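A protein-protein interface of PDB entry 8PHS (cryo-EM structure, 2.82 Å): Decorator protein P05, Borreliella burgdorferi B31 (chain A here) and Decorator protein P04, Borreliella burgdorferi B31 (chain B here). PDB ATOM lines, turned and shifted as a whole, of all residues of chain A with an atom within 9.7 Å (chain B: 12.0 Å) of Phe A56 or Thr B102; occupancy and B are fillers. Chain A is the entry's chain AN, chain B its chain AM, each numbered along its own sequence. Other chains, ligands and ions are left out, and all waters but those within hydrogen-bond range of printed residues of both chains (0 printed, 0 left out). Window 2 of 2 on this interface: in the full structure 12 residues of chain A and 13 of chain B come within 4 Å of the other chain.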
ATOM      1  N   THR A  53     -18.688   9.905  10.678  1.00  0.00           N
ATOM      2  CA  THR A  53     -18.245  11.195  11.180  1.00  0.00           C
ATOM      3  C   THR A  53     -17.364  11.864  10.136  1.00  0.00           C
ATOM      4  O   THR A  53     -16.657  11.196   9.378  1.00  0.00           O
ATOM      5  CB  THR A  53     -17.484  11.048  12.507  1.00  0.00           C
ATOM      6  OG1 THR A  53     -18.236  10.217  13.399  1.00  0.00           O
ATOM      7  CG2 THR A  53     -17.272  12.403  13.165  1.00  0.00           C
ATOM      8  N   SER A  54     -17.416  13.190  10.106  1.00  0.00           N
ATOM      9  CA  SER A  54     -16.600  13.995   9.212  1.00  0.00           C
ATOM     10  C   SER A  54     -15.586  14.796  10.016  1.00  0.00           C
ATOM     11  O   SER A  54     -15.826  15.151  11.174  1.00  0.00           O
ATOM     12  CB  SER A  54     -17.467  14.944   8.380  1.00  0.00           C
ATOM     13  OG  SER A  54     -16.666  15.840   7.632  1.00  0.00           O
ATOM     14  N   LYS A  55     -14.442  15.074   9.388  1.00  0.00           N
ATOM     15  CA  LYS A  55     -13.422  15.890  10.036  1.00  0.00           C
ATOM     16  C   LYS A  55     -13.948  17.280  10.361  1.00  0.00           C
ATOM     17  O   LYS A  55     -13.518  17.896  11.344  1.00  0.00           O
ATOM     18  CB  LYS A  55     -12.182  15.984   9.145  1.00  0.00           C
ATOM     19  CG  LYS A  55     -11.106  16.925   9.660  1.00  0.00           C
ATOM     20  CD  LYS A  55     -10.075  17.228   8.589  1.00  0.00           C
ATOM     21  CE  LYS A  55      -9.064  18.254   9.074  1.00  0.00           C
ATOM     22  NZ  LYS A  55      -8.154  18.697   7.982  1.00  0.00           N
ATOM     23  N   PHE A  56     -14.894  17.779   9.567  1.00  0.00           N
ATOM     24  CA  PHE A  56     -15.408  19.135   9.703  1.00  0.00           C
ATOM     25  C   PHE A  56     -16.683  19.193  10.540  1.00  0.00           C
ATOM     26  O   PHE A  56     -17.527  20.069  10.325  1.00  0.00           O
ATOM     27  CB  PHE A  56     -15.633  19.740   8.320  1.00  0.00           C
ATOM     28  CG  PHE A  56     -14.394  19.767   7.475  1.00  0.00           C
ATOM     29  CD1 PHE A  56     -13.323  20.573   7.818  1.00  0.00           C
ATOM     30  CD2 PHE A  56     -14.288  18.963   6.356  1.00  0.00           C
ATOM     31  CE1 PHE A  56     -12.178  20.591   7.049  1.00  0.00           C
ATOM     32  CE2 PHE A  56     -13.144  18.976   5.583  1.00  0.00           C
ATOM     33  CZ  PHE A  56     -12.088  19.790   5.930  1.00  0.00           C
ATOM     34  N   ASP A  57     -16.835  18.275  11.489  1.00  0.00           N
ATOM     35  CA  ASP A  57     -17.935  18.317  12.441  1.00  0.00           C
ATOM     36  C   ASP A  57     -17.520  19.119  13.667  1.00  0.00           C
ATOM     37  O   ASP A  57     -16.401  18.974  14.167  1.00  0.00           O
ATOM     38  CB  ASP A  57     -18.349  16.905  12.858  1.00  0.00           C
ATOM     39  CG  ASP A  57     -19.046  16.148  11.747  1.00  0.00           C
ATOM     40  OD1 ASP A  57     -19.209  16.718  10.649  1.00  0.00           O
ATOM     41  OD2 ASP A  57     -19.430  14.981  11.971  1.00  0.00           O
ATOM     42  N   LYS A  58     -18.424  19.969  14.145  1.00  0.00           N
ATOM     43  CA  LYS A  58     -18.144  20.827  15.287  1.00  0.00           C
ATOM     44  C   LYS A  58     -18.460  20.094  16.585  1.00  0.00           C
ATOM     45  O   LYS A  58     -19.564  19.570  16.757  1.00  0.00           O
ATOM     46  CB  LYS A  58     -18.949  22.123  15.199  1.00  0.00           C
ATOM     47  CG  LYS A  58     -18.546  23.165  16.224  1.00  0.00           C
ATOM     48  CD  LYS A  58     -19.225  24.496  15.961  1.00  0.00           C
ATOM     49  CE  LYS A  58     -18.612  25.601  16.803  1.00  0.00           C
ATOM     50  NZ  LYS A  58     -19.259  26.915  16.551  1.00  0.00           N
ATOM     51  N   LEU A  59     -17.487  20.065  17.494  1.00  0.00           N
ATOM     52  CA  LEU A  59     -17.616  19.405  18.785  1.00  0.00           C
ATOM     53  C   LEU A  59     -17.308  20.410  19.884  1.00  0.00           C
ATOM     54  O   LEU A  59     -16.303  21.124  19.808  1.00  0.00           O
ATOM     55  CB  LEU A  59     -16.668  18.208  18.884  1.00  0.00           C
ATOM     56  CG  LEU A  59     -16.776  17.158  17.778  1.00  0.00           C
ATOM     57  CD1 LEU A  59     -15.807  16.019  18.028  1.00  0.00           C
ATOM     58  CD2 LEU A  59     -18.194  16.639  17.676  1.00  0.00           C
ATOM     59  N   GLU A  60     -18.163  20.465  20.904  1.00  0.00           N
ATOM     60  CA  GLU A  60     -17.987  21.409  22.001  1.00  0.00           C
ATOM     61  C   GLU A  60     -18.016  20.664  23.325  1.00  0.00           C
ATOM     62  O   GLU A  60     -18.897  19.833  23.549  1.00  0.00           O
ATOM     63  CB  GLU A  60     -19.077  22.484  21.980  1.00  0.00           C
ATOM     64  CG  GLU A  60     -19.190  23.221  20.661  1.00  0.00           C
ATOM     65  CD  GLU A  60     -20.419  24.104  20.588  1.00  0.00           C
ATOM     66  OE1 GLU A  60     -21.208  24.108  21.556  1.00  0.00           O
ATOM     67  OE2 GLU A  60     -20.595  24.793  19.563  1.00  0.00           O
ATOM     68  N   VAL A 116     -22.492  17.727  20.050  1.00  0.00           N
ATOM     69  CA  VAL A 116     -22.673  18.169  18.672  1.00  0.00           C
ATOM     70  C   VAL A 116     -23.848  19.139  18.657  1.00  0.00           C
ATOM     71  O   VAL A 116     -24.962  18.743  19.032  1.00  0.00           O
ATOM     72  CB  VAL A 116     -22.925  16.986  17.727  1.00  0.00           C
ATOM     73  CG1 VAL A 116     -23.127  17.477  16.305  1.00  0.00           C
ATOM     74  CG2 VAL A 116     -21.779  15.996  17.800  1.00  0.00           C
ATOM     75  N   PRO A 117     -23.654  20.392  18.260  1.00  0.00           N
ATOM     76  CA  PRO A 117     -24.761  21.352  18.287  1.00  0.00           C
ATOM     77  C   PRO A 117     -25.856  20.969  17.304  1.00  0.00           C
ATOM     78  O   PRO A 117     -25.642  20.230  16.342  1.00  0.00           O
ATOM     79  CB  PRO A 117     -24.098  22.675  17.890  1.00  0.00           C
ATOM     80  CG  PRO A 117     -22.634  22.460  18.124  1.00  0.00           C
ATOM     81  CD  PRO A 117     -22.393  21.017  17.836  1.00  0.00           C
ATOM     82  N   THR A 119     -27.208  22.582  15.083  1.00  0.00           N
ATOM     83  CA  THR A 119     -26.953  23.066  13.733  1.00  0.00           C
ATOM     84  C   THR A 119     -26.049  22.141  12.930  1.00  0.00           C
ATOM     85  O   THR A 119     -25.779  22.431  11.760  1.00  0.00           O
ATOM     86  CB  THR A 119     -26.331  24.462  13.783  1.00  0.00           C
ATOM     87  OG1 THR A 119     -25.014  24.378  14.340  1.00  0.00           O
ATOM     88  CG2 THR A 119     -27.176  25.382  14.639  1.00  0.00           C
ATOM     89  N   ASN A 120     -25.570  21.052  13.522  1.00  0.00           N
ATOM     90  CA  ASN A 120     -24.721  20.085  12.841  1.00  0.00           C
ATOM     91  C   ASN A 120     -25.442  18.747  12.788  1.00  0.00           C
ATOM     92  O   ASN A 120     -25.950  18.271  13.808  1.00  0.00           O
ATOM     93  CB  ASN A 120     -23.373  19.943  13.553  1.00  0.00           C
ATOM     94  CG  ASN A 120     -22.362  19.160  12.739  1.00  0.00           C
ATOM     95  OD1 ASN A 120     -22.640  18.737  11.618  1.00  0.00           O
ATOM     96  ND2 ASN A 120     -21.176  18.965  13.302  1.00  0.00           N
ATOM     97  N   ASN A 121     -25.492  18.146  11.602  1.00  0.00           N
ATOM     98  CA  ASN A 121     -26.170  16.870  11.434  1.00  0.00           C
ATOM     99  C   ASN A 121     -25.342  15.741  12.035  1.00  0.00           C
ATOM    100  O   ASN A 121     -24.110  15.800  12.085  1.00  0.00           O
ATOM    101  CB  ASN A 121     -26.444  16.596   9.955  1.00  0.00           C
ATOM    102  CG  ASN A 121     -25.179  16.371   9.159  1.00  0.00           C
ATOM    103  OD1 ASN A 121     -24.289  17.219   9.136  1.00  0.00           O
ATOM    104  ND2 ASN A 121     -25.094  15.226   8.495  1.00  0.00           N
ATOM    105  N   TYR B  94     -12.393  40.862  19.841  1.00  0.00           N
ATOM    106  CA  TYR B  94     -12.593  39.707  18.978  1.00  0.00           C
ATOM    107  C   TYR B  94     -13.987  39.139  19.213  1.00  0.00           C
ATOM    108  O   TYR B  94     -14.334  38.771  20.340  1.00  0.00           O
ATOM    109  CB  TYR B  94     -11.512  38.660  19.237  1.00  0.00           C
ATOM    110  CG  TYR B  94     -11.602  37.441  18.350  1.00  0.00           C
ATOM    111  CD1 TYR B  94     -11.206  37.496  17.022  1.00  0.00           C
ATOM    112  CD2 TYR B  94     -12.047  36.230  18.848  1.00  0.00           C
ATOM    113  CE1 TYR B  94     -11.281  36.383  16.208  1.00  0.00           C
ATOM    114  CE2 TYR B  94     -12.118  35.111  18.045  1.00  0.00           C
ATOM    115  CZ  TYR B  94     -11.735  35.192  16.726  1.00  0.00           C
ATOM    116  OH  TYR B  94     -11.807  34.079  15.921  1.00  0.00           O
ATOM    117  N   PHE B  96     -15.729  36.397  18.407  1.00  0.00           N
ATOM    118  CA  PHE B  96     -15.961  35.029  18.858  1.00  0.00           C
ATOM    119  C   PHE B  96     -15.427  34.860  20.273  1.00  0.00           C
ATOM    120  O   PHE B  96     -14.213  34.915  20.493  1.00  0.00           O
ATOM    121  CB  PHE B  96     -15.294  34.015  17.930  1.00  0.00           C
ATOM    122  CG  PHE B  96     -15.829  34.009  16.525  1.00  0.00           C
ATOM    123  CD1 PHE B  96     -15.575  35.062  15.664  1.00  0.00           C
ATOM    124  CD2 PHE B  96     -16.578  32.940  16.065  1.00  0.00           C
ATOM    125  CE1 PHE B  96     -16.059  35.051  14.374  1.00  0.00           C
ATOM    126  CE2 PHE B  96     -17.067  32.925  14.775  1.00  0.00           C
ATOM    127  CZ  PHE B  96     -16.806  33.982  13.929  1.00  0.00           C
ATOM    128  N   CYS B  98     -15.773  31.967  21.830  1.00  0.00           N
ATOM    129  CA  CYS B  98     -15.176  30.651  21.640  1.00  0.00           C
ATOM    130  C   CYS B  98     -15.179  30.354  20.147  1.00  0.00           C
ATOM    131  O   CYS B  98     -16.243  30.149  19.556  1.00  0.00           O
ATOM    132  CB  CYS B  98     -15.944  29.577  22.412  1.00  0.00           C
ATOM    133  SG  CYS B  98     -16.209  29.955  24.158  1.00  0.00           S
ATOM    134  N   SER B  99     -14.000  30.332  19.540  1.00  0.00           N
ATOM    135  CA  SER B  99     -13.891  30.044  18.120  1.00  0.00           C
ATOM    136  C   SER B  99     -13.680  28.553  17.894  1.00  0.00           C
ATOM    137  O   SER B  99     -13.517  27.769  18.832  1.00  0.00           O
ATOM    138  CB  SER B  99     -12.749  30.841  17.488  1.00  0.00           C
ATOM    139  OG  SER B  99     -12.666  30.592  16.098  1.00  0.00           O
ATOM    140  N   SER B 100     -13.682  28.165  16.622  1.00  0.00           N
ATOM    141  CA  SER B 100     -13.504  26.771  16.247  1.00  0.00           C
ATOM    142  C   SER B 100     -13.127  26.706  14.779  1.00  0.00           C
ATOM    143  O   SER B 100     -13.770  27.350  13.946  1.00  0.00           O
ATOM    144  CB  SER B 100     -14.781  25.962  16.497  1.00  0.00           C
ATOM    145  OG  SER B 100     -14.726  24.712  15.832  1.00  0.00           O
ATOM    146  N   TYR B 101     -12.081  25.949  14.464  1.00  0.00           N
ATOM    147  CA  TYR B 101     -11.866  25.590  13.074  1.00  0.00           C
ATOM    148  C   TYR B 101     -13.070  24.787  12.587  1.00  0.00           C
ATOM    149  O   TYR B 101     -13.849  24.248  13.379  1.00  0.00           O
ATOM    150  CB  TYR B 101     -10.559  24.812  12.910  1.00  0.00           C
ATOM    151  CG  TYR B 101     -10.573  23.409  13.464  1.00  0.00           C
ATOM    152  CD1 TYR B 101     -10.359  23.168  14.812  1.00  0.00           C
ATOM    153  CD2 TYR B 101     -10.755  22.319  12.626  1.00  0.00           C
ATOM    154  CE1 TYR B 101     -10.363  21.881  15.314  1.00  0.00           C
ATOM    155  CE2 TYR B 101     -10.762  21.031  13.115  1.00  0.00           C
ATOM    156  CZ  TYR B 101     -10.563  20.816  14.458  1.00  0.00           C
ATOM    157  OH  TYR B 101     -10.566  19.530  14.943  1.00  0.00           O
ATOM    158  N   THR B 102     -13.233  24.736  11.264  1.00  0.00           N
ATOM    159  CA  THR B 102     -14.433  24.264  10.572  1.00  0.00           C
ATOM    160  C   THR B 102     -15.609  25.218  10.727  1.00  0.00           C
ATOM    161  O   THR B 102     -16.757  24.814  10.510  1.00  0.00           O
ATOM    162  CB  THR B 102     -14.872  22.856  11.000  1.00  0.00           C
ATOM    163  OG1 THR B 102     -15.504  22.916  12.285  1.00  0.00           O
ATOM    164  CG2 THR B 102     -13.690  21.907  11.051  1.00  0.00           C
ATOM    165  N   ASP B 103     -15.361  26.468  11.110  1.00  0.00           N
ATOM    166  CA  ASP B 103     -16.375  27.511  11.038  1.00  0.00           C
ATOM    167  C   ASP B 103     -16.261  28.213   9.692  1.00  0.00           C
ATOM    168  O   ASP B 103     -15.178  28.669   9.312  1.00  0.00           O
ATOM    169  CB  ASP B 103     -16.217  28.521  12.176  1.00  0.00           C
ATOM    170  CG  ASP B 103     -16.745  27.999  13.498  1.00  0.00           C
ATOM    171  OD1 ASP B 103     -17.677  27.170  13.482  1.00  0.00           O
ATOM    172  OD2 ASP B 103     -16.241  28.433  14.555  1.00  0.00           O
ATOM    173  N   LYS B 104     -17.377  28.297   8.975  1.00  0.00           N
ATOM    174  CA  LYS B 104     -17.397  28.865   7.634  1.00  0.00           C
ATOM    175  C   LYS B 104     -17.563  30.377   7.711  1.00  0.00           C
ATOM    176  O   LYS B 104     -18.491  30.874   8.355  1.00  0.00           O
ATOM    177  CB  LYS B 104     -18.527  28.245   6.812  1.00  0.00           C
ATOM    178  CG  LYS B 104     -18.596  28.724   5.375  1.00  0.00           C
ATOM    179  CD  LYS B 104     -19.423  27.771   4.530  1.00  0.00           C
ATOM    180  CE  LYS B 104     -19.559  28.267   3.100  1.00  0.00           C
ATOM    181  NZ  LYS B 104     -20.274  27.286   2.240  1.00  0.00           N
ATOM    182  N   ILE B 105     -16.661  31.102   7.055  1.00  0.00           N
ATOM    183  CA  ILE B 105     -16.682  32.559   7.017  1.00  0.00           C
ATOM    184  C   ILE B 105     -16.717  32.994   5.559  1.00  0.00           C
ATOM    185  O   ILE B 105     -15.922  32.512   4.744  1.00  0.00           O
ATOM    186  CB  ILE B 105     -15.465  33.162   7.741  1.00  0.00           C
ATOM    187  CG1 ILE B 105     -15.342  32.576   9.148  1.00  0.00           C
ATOM    188  CG2 ILE B 105     -15.580  34.675   7.807  1.00  0.00           C
ATOM    189  CD1 ILE B 105     -14.025  32.877   9.824  1.00  0.00           C
ATOM    190  N   GLU B 106     -17.632  33.903   5.232  1.00  0.00           N
ATOM    191  CA  GLU B 106     -17.823  34.362   3.865  1.00  0.00           C
ATOM    192  C   GLU B 106     -17.573  35.862   3.778  1.00  0.00           C
ATOM    193  O   GLU B 106     -17.691  36.590   4.764  1.00  0.00           O
ATOM    194  CB  GLU B 106     -19.237  34.040   3.369  1.00  0.00           C
ATOM    195  CG  GLU B 106     -19.486  32.563   3.127  1.00  0.00           C
ATOM    196  CD  GLU B 106     -20.927  32.266   2.770  1.00  0.00           C
ATOM    197  OE1 GLU B 106     -21.765  33.187   2.861  1.00  0.00           O
ATOM    198  OE2 GLU B 106     -21.223  31.112   2.397  1.00  0.00           O
ATOM    199  N   VAL B 157     -18.975  37.396   7.187  1.00  0.00           N
ATOM    200  CA  VAL B 157     -20.256  36.898   7.665  1.00  0.00           C
ATOM    201  C   VAL B 157     -20.101  35.443   8.082  1.00  0.00           C
ATOM    202  O   VAL B 157     -19.510  34.638   7.351  1.00  0.00           O
ATOM    203  CB  VAL B 157     -21.352  37.041   6.592  1.00  0.00           C
ATOM    204  CG1 VAL B 157     -22.690  36.568   7.132  1.00  0.00           C
ATOM    205  CG2 VAL B 157     -21.443  38.481   6.116  1.00  0.00           C
ATOM    206  N   LEU B 158     -20.618  35.122   9.265  1.00  0.00           N
ATOM    207  CA  LEU B 158     -20.816  33.754   9.705  1.00  0.00           C
ATOM    208  C   LEU B 158     -22.247  33.364   9.375  1.00  0.00           C
ATOM    209  O   LEU B 158     -23.181  33.983   9.909  1.00  0.00           O
ATOM    210  CB  LEU B 158     -20.563  33.631  11.205  1.00  0.00           C
ATOM    211  CG  LEU B 158     -20.664  32.245  11.843  1.00  0.00           C
ATOM    212  CD1 LEU B 158     -19.623  31.306  11.270  1.00  0.00           C
ATOM    213  CD2 LEU B 158     -20.531  32.343  13.353  1.00  0.00           C
ATOM    214  N   PRO B 159     -22.473  32.389   8.496  1.00  0.00           N
ATOM    215  CA  PRO B 159     -23.846  32.021   8.135  1.00  0.00           C
ATOM    216  C   PRO B 159     -24.633  31.519   9.334  1.00  0.00           C
ATOM    217  O   PRO B 159     -24.077  30.968  10.287  1.00  0.00           O
ATOM    218  CB  PRO B 159     -23.649  30.912   7.096  1.00  0.00           C
ATOM    219  CG  PRO B 159     -22.333  31.225   6.481  1.00  0.00           C
ATOM    220  CD  PRO B 159     -21.485  31.767   7.600  1.00  0.00           C
ATOM    221  N   ILE B 160     -25.952  31.723   9.277  1.00  0.00           N
ATOM    222  CA  ILE B 160     -26.835  31.311  10.360  1.00  0.00           C
ATOM    223  C   ILE B 160     -26.808  29.803  10.569  1.00  0.00           C
ATOM    224  O   ILE B 160     -27.156  29.322  11.653  1.00  0.00           O
ATOM    225  CB  ILE B 160     -28.270  31.811  10.087  1.00  0.00           C
ATOM    226  CG1 ILE B 160     -29.144  31.664  11.334  1.00  0.00           C
ATOM    227  CG2 ILE B 160     -28.881  31.073   8.906  1.00  0.00           C
ATOM    228  CD1 ILE B 160     -30.457  32.401  11.246  1.00  0.00           C
ATOM    229  N   THR B 161     -26.393  29.038   9.558  1.00  0.00           N
ATOM    230  CA  THR B 161     -26.290  27.591   9.711  1.00  0.00           C
ATOM    231  C   THR B 161     -25.205  27.183  10.700  1.00  0.00           C
ATOM    232  O   THR B 161     -25.194  26.030  11.143  1.00  0.00           O
ATOM    233  CB  THR B 161     -26.023  26.932   8.356  1.00  0.00           C
ATOM    234  OG1 THR B 161     -24.829  27.477   7.784  1.00  0.00           O
ATOM    235  CG2 THR B 161     -27.184  27.170   7.410  1.00  0.00           C
ATOM    236  N   ASN B 162     -24.294  28.087  11.045  1.00  0.00           N
ATOM    237  CA  ASN B 162     -23.240  27.802  12.006  1.00  0.00           C
ATOM    238  C   ASN B 162     -23.570  28.405  13.364  1.00  0.00           C
ATOM    239  O   ASN B 162     -24.255  29.425  13.463  1.00  0.00           O
ATOM    240  CB  ASN B 162     -21.892  28.340  11.523  1.00  0.00           C
ATOM    241  CG  ASN B 162     -21.412  27.666  10.257  1.00  0.00           C
ATOM    242  OD1 ASN B 162     -22.101  26.818   9.691  1.00  0.00           O
ATOM    243  ND2 ASN B 162     -20.219  28.035   9.810  1.00  0.00           N
ATOM    244  N   ASN B 163     -23.074  27.757  14.413  1.00  0.00           N
ATOM    245  CA  ASN B 163     -23.242  28.265  15.762  1.00  0.00           C
ATOM    246  C   ASN B 163     -22.394  29.512  15.977  1.00  0.00           C
ATOM    247  O   ASN B 163     -21.391  29.743  15.295  1.00  0.00           O
ATOM    248  CB  ASN B 163     -22.854  27.203  16.787  1.00  0.00           C
ATOM    249  CG  ASN B 163     -23.569  25.902  16.560  1.00  0.00           C
ATOM    250  OD1 ASN B 163     -22.978  24.934  16.089  1.00  0.00           O
ATOM    251  ND2 ASN B 163     -24.851  25.867  16.895  1.00  0.00           N
ATOM    252  N   PHE B 164     -22.811  30.322  16.942  1.00  0.00           N
ATOM    253  CA  PHE B 164     -22.064  31.509  17.322  1.00  0.00           C
ATOM    254  C   PHE B 164     -22.183  31.707  18.823  1.00  0.00           C
ATOM    255  O   PHE B 164     -23.234  31.442  19.408  1.00  0.00           O
ATOM    256  CB  PHE B 164     -22.573  32.753  16.585  1.00  0.00           C
ATOM    257  CG  PHE B 164     -21.815  34.005  16.916  1.00  0.00           C
ATOM    258  CD1 PHE B 164     -20.519  34.182  16.466  1.00  0.00           C
ATOM    259  CD2 PHE B 164     -22.398  35.006  17.672  1.00  0.00           C
ATOM    260  CE1 PHE B 164     -19.818  35.332  16.765  1.00  0.00           C
ATOM    261  CE2 PHE B 164     -21.702  36.161  17.974  1.00  0.00           C
ATOM    262  CZ  PHE B 164     -20.410  36.322  17.520  1.00  0.00           C
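OG of Ser A54 lies close to N of Phe A56 (3.3 Å).
The backbone NH of Ser B100 is in hydrogen-bond range of the side-chain carboxylate of Asp B103 (3.3 Å).
ND2 of Asn A120 sits close to N of Lys A58, 3.0 Å away.
The side-chain amino group of Lys A58 lies within salt-bridge range of the side-chain carboxylate of Glu A60 (3.9 Å).
OG1 of Thr B161 sits close to OD1 of Asn B162 (3.4 Å).
Thr B102 touches Phe A56.
Lys A58 touches Ser B100 (CE to CB, 3.9 Å).
Lys A58 touches Asn B163.
Pro A117 touches Asn B163 (CB to OD1, 3.1 Å).
Thr A119 touches Thr B161.
The side-chain amino group (NZ) of Lys A58 is in salt-bridge range of the side-chain carboxylate (OD1) of Asp B103 (3.5 Å).
OG1 of Thr A119 is in hydrogen-bond range of OD1 of Asn B163 (2.7 Å).
Printed residues of chain B within 4 Å of Phe A56: Thr B102 (3.5 Å).
Ser A54 touches none of the printed residues of chain B.
No residue of chain B comes within 4 Å of Asp A57.
Lys A58 touches three residues of chain B.
Of chain A, only Lys A58 (3.5 Å) comes within 4 Å of Asp B103.
Of the printed residues of chain A, Asn B163 touches Lys A58 (3.6 Å), Pro A117 (3.1 Å) and Thr A119 (2.7 Å).
Of the printed residues of chain B, Pro A117 touches Asn B163 (3.1 Å).
Printed residues of chain A within 4 Å of Ser B100: Lys A58 (3.9 Å).
Ile B105 touches none of the printed residues of chain A.
Leu A59 touches none of the printed residues of chain B.
Of the 19 printed residues of chain B, 5 touch a printed residue of chain A.
Printed residues of chain B that touch a printed residue of chain A: Ser B100, Thr B102, Asp B103, Thr B161 and Asn B163.
Hydrophobic or aromatic side chains of chain A within 4 Å of the printed part of chain B: Phe A56 and Pro A117.
Along chain A the printed residues that touch a printed residue of chain B span positions 56 to 119.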
